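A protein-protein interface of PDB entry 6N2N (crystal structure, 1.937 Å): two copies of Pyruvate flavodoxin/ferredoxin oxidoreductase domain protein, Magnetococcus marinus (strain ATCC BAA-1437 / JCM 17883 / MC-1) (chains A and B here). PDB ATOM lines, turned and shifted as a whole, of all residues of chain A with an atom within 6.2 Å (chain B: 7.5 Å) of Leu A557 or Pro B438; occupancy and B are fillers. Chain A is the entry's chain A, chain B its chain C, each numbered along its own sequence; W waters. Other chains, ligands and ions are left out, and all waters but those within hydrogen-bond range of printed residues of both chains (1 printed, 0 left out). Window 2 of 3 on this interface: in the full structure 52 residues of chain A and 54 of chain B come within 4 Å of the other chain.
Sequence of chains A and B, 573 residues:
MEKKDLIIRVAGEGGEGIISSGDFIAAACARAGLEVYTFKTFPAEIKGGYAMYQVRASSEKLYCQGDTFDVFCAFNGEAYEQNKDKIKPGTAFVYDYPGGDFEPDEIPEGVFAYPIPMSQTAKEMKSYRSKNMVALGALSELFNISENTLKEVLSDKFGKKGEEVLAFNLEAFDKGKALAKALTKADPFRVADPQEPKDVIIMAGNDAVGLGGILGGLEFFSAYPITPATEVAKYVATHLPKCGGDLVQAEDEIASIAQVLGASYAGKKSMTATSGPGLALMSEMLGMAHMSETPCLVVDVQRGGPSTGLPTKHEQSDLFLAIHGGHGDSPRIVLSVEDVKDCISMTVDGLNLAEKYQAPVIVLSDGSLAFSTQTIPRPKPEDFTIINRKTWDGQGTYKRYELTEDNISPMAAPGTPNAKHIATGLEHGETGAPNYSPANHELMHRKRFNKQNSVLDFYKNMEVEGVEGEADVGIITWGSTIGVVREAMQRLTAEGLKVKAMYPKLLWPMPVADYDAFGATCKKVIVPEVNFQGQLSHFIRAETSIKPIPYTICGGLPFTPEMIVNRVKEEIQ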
ATOM      1  N   LEU A 310      12.006  -4.916 -13.501  1.00  0.00           N
ATOM      2  CA  LEU A 310      13.369  -5.439 -13.618  1.00  0.00           C
ATOM      3  C   LEU A 310      13.269  -6.721 -14.434  1.00  0.00           C
ATOM      4  O   LEU A 310      13.175  -7.826 -13.876  1.00  0.00           O
ATOM      5  CB  LEU A 310      14.006  -5.694 -12.247  1.00  0.00           C
ATOM      6  CG  LEU A 310      14.046  -4.571 -11.202  1.00  0.00           C
ATOM      7  CD1 LEU A 310      12.697  -4.433 -10.477  1.00  0.00           C
ATOM      8  CD2 LEU A 310      15.155  -4.805 -10.195  1.00  0.00           C
ATOM      9  N   LYS A 313      15.657  -9.809 -13.621  1.00  0.00           N
ATOM     10  CA  LYS A 313      15.964 -10.133 -12.239  1.00  0.00           C
ATOM     11  C   LYS A 313      14.984 -11.164 -11.681  1.00  0.00           C
ATOM     12  O   LYS A 313      14.012 -11.563 -12.331  1.00  0.00           O
ATOM     13  CB  LYS A 313      15.965  -8.862 -11.394  1.00  0.00           C
ATOM     14  CG  LYS A 313      17.010  -7.853 -11.844  1.00  0.00           C
ATOM     15  CD  LYS A 313      18.382  -8.533 -11.999  1.00  0.00           C
ATOM     16  CE  LYS A 313      19.471  -7.508 -12.284  1.00  0.00           C
ATOM     17  NZ  LYS A 313      20.815  -8.144 -12.286  1.00  0.00           N
ATOM     18  N   HIS A 314      15.234 -11.574 -10.439  1.00  0.00           N
ATOM     19  CA  HIS A 314      14.488 -12.649  -9.798  1.00  0.00           C
ATOM     20  C   HIS A 314      13.386 -12.089  -8.910  1.00  0.00           C
ATOM     21  O   HIS A 314      13.651 -11.265  -8.029  1.00  0.00           O
ATOM     22  CB  HIS A 314      15.406 -13.535  -8.956  1.00  0.00           C
ATOM     23  CG  HIS A 314      14.698 -14.701  -8.346  1.00  0.00           C
ATOM     24  ND1 HIS A 314      14.654 -15.939  -8.947  1.00  0.00           N
ATOM     25  CD2 HIS A 314      13.980 -14.810  -7.203  1.00  0.00           C
ATOM     26  CE1 HIS A 314      13.940 -16.763  -8.200  1.00  0.00           C
ATOM     27  NE2 HIS A 314      13.524 -16.104  -7.134  1.00  0.00           N
ATOM     28  N   GLU A 315      12.167 -12.584  -9.099  1.00  0.00           N
ATOM     29  CA  GLU A 315      11.039 -12.130  -8.296  1.00  0.00           C
ATOM     30  C   GLU A 315       9.874 -13.086  -8.500  1.00  0.00           C
ATOM     31  O   GLU A 315       9.681 -13.605  -9.605  1.00  0.00           O
ATOM     32  CB  GLU A 315      10.631 -10.701  -8.685  1.00  0.00           C
ATOM     33  CG  GLU A 315       9.902  -9.928  -7.600  1.00  0.00           C
ATOM     34  CD  GLU A 315       9.818  -8.440  -7.917  1.00  0.00           C
ATOM     35  OE1 GLU A 315       8.754  -7.989  -8.404  1.00  0.00           O
ATOM     36  OE2 GLU A 315      10.821  -7.725  -7.698  1.00  0.00           O
ATOM     37  N   VAL A 530      10.046 -14.142  -2.408  1.00  0.00           N
ATOM     38  CA  VAL A 530      10.639 -12.961  -3.027  1.00  0.00           C
ATOM     39  C   VAL A 530       9.538 -12.087  -3.618  1.00  0.00           C
ATOM     40  O   VAL A 530       9.280 -12.109  -4.827  1.00  0.00           O
ATOM     41  CB  VAL A 530      11.691 -13.341  -4.088  1.00  0.00           C
ATOM     42  CG1 VAL A 530      12.489 -12.102  -4.514  1.00  0.00           C
ATOM     43  CG2 VAL A 530      12.637 -14.404  -3.541  1.00  0.00           C
ATOM     44  N   ILE A 553      11.891 -10.684   0.902  1.00  0.00           N
ATOM     45  CA  ILE A 553      12.938  -9.894   0.274  1.00  0.00           C
ATOM     46  C   ILE A 553      12.443  -9.527  -1.114  1.00  0.00           C
ATOM     47  O   ILE A 553      11.590 -10.213  -1.687  1.00  0.00           O
ATOM     48  CB  ILE A 553      14.296 -10.635   0.208  1.00  0.00           C
ATOM     49  CG1 ILE A 553      14.217 -11.825  -0.754  1.00  0.00           C
ATOM     50  CG2 ILE A 553      14.732 -11.085   1.611  1.00  0.00           C
ATOM     51  CD1 ILE A 553      15.511 -12.619  -0.864  1.00  0.00           C
ATOM     52  N   CYS A 554      12.951  -8.417  -1.643  1.00  0.00           N
ATOM     53  CA  CYS A 554      12.545  -7.969  -2.969  1.00  0.00           C
ATOM     54  C   CYS A 554      13.636  -7.093  -3.567  1.00  0.00           C
ATOM     55  O   CYS A 554      13.447  -5.885  -3.747  1.00  0.00           O
ATOM     56  CB  CYS A 554      11.206  -7.217  -2.905  1.00  0.00           C
ATOM     57  SG  CYS A 554      10.278  -7.155  -4.485  1.00  0.00           S
ATOM     58  N   GLY A 555      14.780  -7.698  -3.875  1.00  0.00           N
ATOM     59  CA  GLY A 555      15.904  -6.972  -4.432  1.00  0.00           C
ATOM     60  C   GLY A 555      16.372  -7.565  -5.745  1.00  0.00           C
ATOM     61  O   GLY A 555      17.508  -7.342  -6.159  1.00  0.00           O
ATOM     62  N   GLY A 556      15.506  -8.328  -6.410  1.00  0.00           N
ATOM     63  CA  GLY A 556      15.863  -8.945  -7.668  1.00  0.00           C
ATOM     64  C   GLY A 556      16.737 -10.177  -7.559  1.00  0.00           C
ATOM     65  O   GLY A 556      17.217 -10.667  -8.589  1.00  0.00           O
ATOM     66  N   LEU A 557      16.951 -10.701  -6.351  1.00  0.00           N
ATOM     67  CA  LEU A 557      17.772 -11.884  -6.125  1.00  0.00           C
ATOM     68  C   LEU A 557      16.978 -12.971  -5.409  1.00  0.00           C
ATOM     69  O   LEU A 557      16.081 -12.670  -4.618  1.00  0.00           O
ATOM     70  CB  LEU A 557      19.016 -11.548  -5.287  1.00  0.00           C
ATOM     71  CG  LEU A 557      20.033 -10.564  -5.865  1.00  0.00           C
ATOM     72  CD1 LEU A 557      21.022 -10.130  -4.794  1.00  0.00           C
ATOM     73  CD2 LEU A 557      20.755 -11.206  -7.038  1.00  0.00           C
ATOM     74  N   PRO A 558      17.291 -14.242  -5.651  1.00  0.00           N
ATOM     75  CA  PRO A 558      16.679 -15.318  -4.864  1.00  0.00           C
ATOM     76  C   PRO A 558      17.271 -15.385  -3.463  1.00  0.00           C
ATOM     77  O   PRO A 558      18.318 -14.807  -3.163  1.00  0.00           O
ATOM     78  CB  PRO A 558      17.017 -16.574  -5.669  1.00  0.00           C
ATOM     79  CG  PRO A 558      18.332 -16.231  -6.319  1.00  0.00           C
ATOM     80  CD  PRO A 558      18.240 -14.759  -6.655  1.00  0.00           C
ATOM     81  N   PHE A 559      16.572 -16.109  -2.592  1.00  0.00           N
ATOM     82  CA  PHE A 559      17.144 -16.505  -1.313  1.00  0.00           C
ATOM     83  C   PHE A 559      18.321 -17.454  -1.525  1.00  0.00           C
ATOM     84  O   PHE A 559      18.418 -18.146  -2.538  1.00  0.00           O
ATOM     85  CB  PHE A 559      16.107 -17.220  -0.445  1.00  0.00           C
ATOM     86  CG  PHE A 559      15.053 -16.320   0.121  1.00  0.00           C
ATOM     87  CD1 PHE A 559      15.255 -15.676   1.333  1.00  0.00           C
ATOM     88  CD2 PHE A 559      13.848 -16.148  -0.534  1.00  0.00           C
ATOM     89  CE1 PHE A 559      14.279 -14.852   1.870  1.00  0.00           C
ATOM     90  CE2 PHE A 559      12.871 -15.336  -0.005  1.00  0.00           C
ATOM     91  CZ  PHE A 559      13.092 -14.680   1.200  1.00  0.00           C
ATOM     92  N   ASN B 435      17.557   1.337 -12.975  1.00  0.00           N
ATOM     93  CA  ASN B 435      18.403   0.912 -11.861  1.00  0.00           C
ATOM     94  C   ASN B 435      17.872  -0.437 -11.400  1.00  0.00           C
ATOM     95  O   ASN B 435      16.753  -0.503 -10.885  1.00  0.00           O
ATOM     96  CB  ASN B 435      18.371   1.945 -10.734  1.00  0.00           C
ATOM     97  CG  ASN B 435      19.359   1.641  -9.604  1.00  0.00           C
ATOM     98  OD1 ASN B 435      19.571   0.489  -9.221  1.00  0.00           O
ATOM     99  ND2 ASN B 435      19.969   2.692  -9.070  1.00  0.00           N
ATOM    100  N   TYR B 436      18.654  -1.504 -11.588  1.00  0.00           N
ATOM    101  CA  TYR B 436      18.212  -2.856 -11.251  1.00  0.00           C
ATOM    102  C   TYR B 436      18.924  -3.415 -10.027  1.00  0.00           C
ATOM    103  O   TYR B 436      18.868  -4.626  -9.788  1.00  0.00           O
ATOM    104  CB  TYR B 436      18.411  -3.803 -12.438  1.00  0.00           C
ATOM    105  CG  TYR B 436      17.904  -3.243 -13.743  1.00  0.00           C
ATOM    106  CD1 TYR B 436      16.572  -2.907 -13.904  1.00  0.00           C
ATOM    107  CD2 TYR B 436      18.770  -3.018 -14.803  1.00  0.00           C
ATOM    108  CE1 TYR B 436      16.109  -2.378 -15.094  1.00  0.00           C
ATOM    109  CE2 TYR B 436      18.318  -2.488 -15.995  1.00  0.00           C
ATOM    110  CZ  TYR B 436      16.988  -2.169 -16.135  1.00  0.00           C
ATOM    111  OH  TYR B 436      16.535  -1.644 -17.324  1.00  0.00           O
ATOM    112  N   SER B 437      19.597  -2.563  -9.258  1.00  0.00           N
ATOM    113  CA  SER B 437      20.352  -3.036  -8.114  1.00  0.00           C
ATOM    114  C   SER B 437      19.409  -3.460  -6.987  1.00  0.00           C
ATOM    115  O   SER B 437      18.310  -2.915  -6.841  1.00  0.00           O
ATOM    116  CB  SER B 437      21.308  -1.949  -7.625  1.00  0.00           C
ATOM    117  OG  SER B 437      20.592  -0.854  -7.085  1.00  0.00           O
ATOM    118  N   PRO B 438      19.814  -4.446  -6.184  1.00  0.00           N
ATOM    119  CA  PRO B 438      18.937  -4.894  -5.089  1.00  0.00           C
ATOM    120  C   PRO B 438      18.571  -3.790  -4.116  1.00  0.00           C
ATOM    121  O   PRO B 438      17.386  -3.613  -3.798  1.00  0.00           O
ATOM    122  CB  PRO B 438      19.764  -6.002  -4.422  1.00  0.00           C
ATOM    123  CG  PRO B 438      20.686  -6.492  -5.504  1.00  0.00           C
ATOM    124  CD  PRO B 438      21.035  -5.268  -6.297  1.00  0.00           C
ATOM    125  N   ALA B 439      19.556  -3.023  -3.645  1.00  0.00           N
ATOM    126  CA  ALA B 439      19.274  -2.008  -2.634  1.00  0.00           C
ATOM    127  C   ALA B 439      18.292  -0.962  -3.148  1.00  0.00           C
ATOM    128  O   ALA B 439      17.441  -0.474  -2.393  1.00  0.00           O
ATOM    129  CB  ALA B 439      20.575  -1.343  -2.179  1.00  0.00           C
ATOM    130  N   ASN B 440      18.387  -0.606  -4.431  1.00  0.00           N
ATOM    131  CA  ASN B 440      17.509   0.438  -4.948  1.00  0.00           C
ATOM    132  C   ASN B 440      16.072  -0.056  -5.065  1.00  0.00           C
ATOM    133  O   ASN B 440      15.130   0.700  -4.803  1.00  0.00           O
ATOM    134  CB  ASN B 440      18.013   0.952  -6.296  1.00  0.00           C
ATOM    135  CG  ASN B 440      17.095   2.009  -6.885  1.00  0.00           C
ATOM    136  OD1 ASN B 440      17.140   3.174  -6.486  1.00  0.00           O
ATOM    137  ND2 ASN B 440      16.246   1.608  -7.829  1.00  0.00           N
ATOM    138  N   HIS B 441      15.882  -1.310  -5.486  1.00  0.00           N
ATOM    139  CA  HIS B 441      14.536  -1.867  -5.586  1.00  0.00           C
ATOM    140  C   HIS B 441      13.866  -1.921  -4.218  1.00  0.00           C
ATOM    141  O   HIS B 441      12.700  -1.529  -4.066  1.00  0.00           O
ATOM    142  CB  HIS B 441      14.597  -3.258  -6.222  1.00  0.00           C
ATOM    143  CG  HIS B 441      13.270  -3.771  -6.694  1.00  0.00           C
ATOM    144  ND1 HIS B 441      12.291  -2.948  -7.206  1.00  0.00           N
ATOM    145  CD2 HIS B 441      12.776  -5.031  -6.764  1.00  0.00           C
ATOM    146  CE1 HIS B 441      11.239  -3.673  -7.544  1.00  0.00           C
ATOM    147  NE2 HIS B 441      11.510  -4.941  -7.291  1.00  0.00           N
ATOM    148  N   GLU B 442      14.602  -2.391  -3.205  1.00  0.00           N
ATOM    149  CA  GLU B 442      14.086  -2.395  -1.838  1.00  0.00           C
ATOM    150  C   GLU B 442      13.748  -0.987  -1.374  1.00  0.00           C
ATOM    151  O   GLU B 442      12.708  -0.759  -0.746  1.00  0.00           O
ATOM    152  CB  GLU B 442      15.116  -3.017  -0.895  1.00  0.00           C
ATOM    153  CG  GLU B 442      15.460  -4.456  -1.190  1.00  0.00           C
ATOM    154  CD  GLU B 442      14.516  -5.428  -0.509  1.00  0.00           C
ATOM    155  OE1 GLU B 442      13.428  -4.992  -0.059  1.00  0.00           O
ATOM    156  OE2 GLU B 442      14.874  -6.624  -0.416  1.00  0.00           O
ATOM    157  N   LEU B 443      14.625  -0.034  -1.678  1.00  0.00           N
ATOM    158  CA  LEU B 443      14.447   1.342  -1.237  1.00  0.00           C
ATOM    159  C   LEU B 443      13.259   1.999  -1.933  1.00  0.00           C
ATOM    160  O   LEU B 443      12.489   2.727  -1.297  1.00  0.00           O
ATOM    161  CB  LEU B 443      15.745   2.115  -1.501  1.00  0.00           C
ATOM    162  CG  LEU B 443      15.966   3.554  -1.048  1.00  0.00           C
ATOM    163  CD1 LEU B 443      15.186   4.528  -1.927  1.00  0.00           C
ATOM    164  CD2 LEU B 443      15.624   3.732   0.425  1.00  0.00           C
ATOM    165  N   MET B 444      13.103   1.773  -3.243  1.00  0.00           N
ATOM    166  CA  MET B 444      12.027   2.427  -3.979  1.00  0.00           C
ATOM    167  C   MET B 444      10.677   1.777  -3.726  1.00  0.00           C
ATOM    168  O   MET B 444       9.656   2.469  -3.722  1.00  0.00           O
ATOM    169  CB  MET B 444      12.335   2.441  -5.475  1.00  0.00           C
ATOM    170  CG  MET B 444      13.418   3.452  -5.863  1.00  0.00           C
ATOM    171  SD  MET B 444      12.891   5.167  -5.576  1.00  0.00           S
ATOM    172  CE  MET B 444      14.264   6.048  -6.301  1.00  0.00           C
ATOM    173  N   ARG B 446       9.866   0.671  -0.789  1.00  0.00           N
ATOM    174  CA  ARG B 446       9.511   1.310   0.471  1.00  0.00           C
ATOM    175  C   ARG B 446       9.075   2.757   0.263  1.00  0.00           C
ATOM    176  O   ARG B 446       8.177   3.239   0.955  1.00  0.00           O
ATOM    177  CB  ARG B 446      10.684   1.216   1.452  1.00  0.00           C
ATOM    178  CG  ARG B 446      10.805  -0.168   2.095  1.00  0.00           C
ATOM    179  CD  ARG B 446      12.123  -0.365   2.858  1.00  0.00           C
ATOM    180  NE  ARG B 446      12.159  -1.679   3.506  1.00  0.00           N
ATOM    181  CZ  ARG B 446      12.416  -2.824   2.877  1.00  0.00           C
ATOM    182  NH1 ARG B 446      12.671  -2.827   1.575  1.00  0.00           N
ATOM    183  NH2 ARG B 446      12.426  -3.969   3.551  1.00  0.00           N
HETATM  184  O   HOH W   1      18.708  -7.081  -8.521  1.00  0.00           O
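Printed residues of chain A that touch a printed residue of chain B: Leu A310, Lys A313, Glu A315, Ile A553, Cys A554, Gly A555 and Leu A557.
Hydrophobic or aromatic side chains of chain A within 4 Å of the printed part of chain B: Leu A310 and Leu A557.
Hydrophobic or aromatic side chains of chain B that line the printed part of chain A: Tyr B436, Pro B438 and His B441.
Among the printed residues, no Asp or Glu carboxylate lies within 4 Å of a Lys or Arg side-chain nitrogen of the other chain.
NE2 of His B441 lies within hydrogen-bond range of OE2 of Glu A315, 2.9 Å away.
NE2 of His B441 lies within hydrogen-bond range of SG of Cys A554, 3.8 Å away.
The side-chain carboxylate (OE2) of Glu B442 sits at hydrogen-bond distance from the backbone NH (N) of Cys A554, at 2.9 Å.
SG of Cys A554 lies within hydrogen-bond range of OE2 of Glu A315, 3.3 Å away.
NH1 of Arg B446 lies within salt-bridge range of OE1 of Glu B442 (2.8 Å).
Water W1 lies within hydrogen-bond range of the backbone carbonyl oxygen (O) of Gly A555 (2.7 Å) and the backbone carbonyl oxygen (O) of Tyr B436 (2.8 Å).
Among the printed residues, pairs that only touch across the chains: Leu A310 with Tyr B436 (3.7 Å), Leu A310 with His B441 (3.4 Å), Lys A313 with Tyr B436 (3.9 Å), Ile A553 with Glu B442 (3.9 Å), Gly A555 with Pro B438 (3.0 Å), Gly A555 with Glu B442 (3.6 Å) and Leu A557 with Pro B438 (3.7 Å).
No position is printed for both chains.
Of the 10 pairs that touch across the chains among the printed residues, none has its exchanged pair printed and touching as well.
Of the printed residues of chain B, Glu A315 touches His B441 (2.9 Å).
Of the printed residues of chain B, Ile A553 touches Glu B442 (3.9 Å).
Of the printed residues of chain B, Cys A554 touches His B441 and Glu B442.
Gly A556 touches none of the printed residues of chain B.
Of chain B, only Pro B438 (3.7 Å) comes within 4 Å of Leu A557.
Asn B435 touches none of the printed residues of chain A.
Of chain A, only Gly A555 and Leu A557 come within 4 Å of Pro B438.
Printed residues of chain A within 4 Å of Glu B442: Ile A553, Cys A554 and Gly A555.
Met B444 touches none of the printed residues of chain A.
The nearest residue of chain B that does not touch Leu A557 is His B441 (7.1 Å).
The nearest residue of chain A that does not touch Pro B438 is Cys A554 (4.5 Å).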
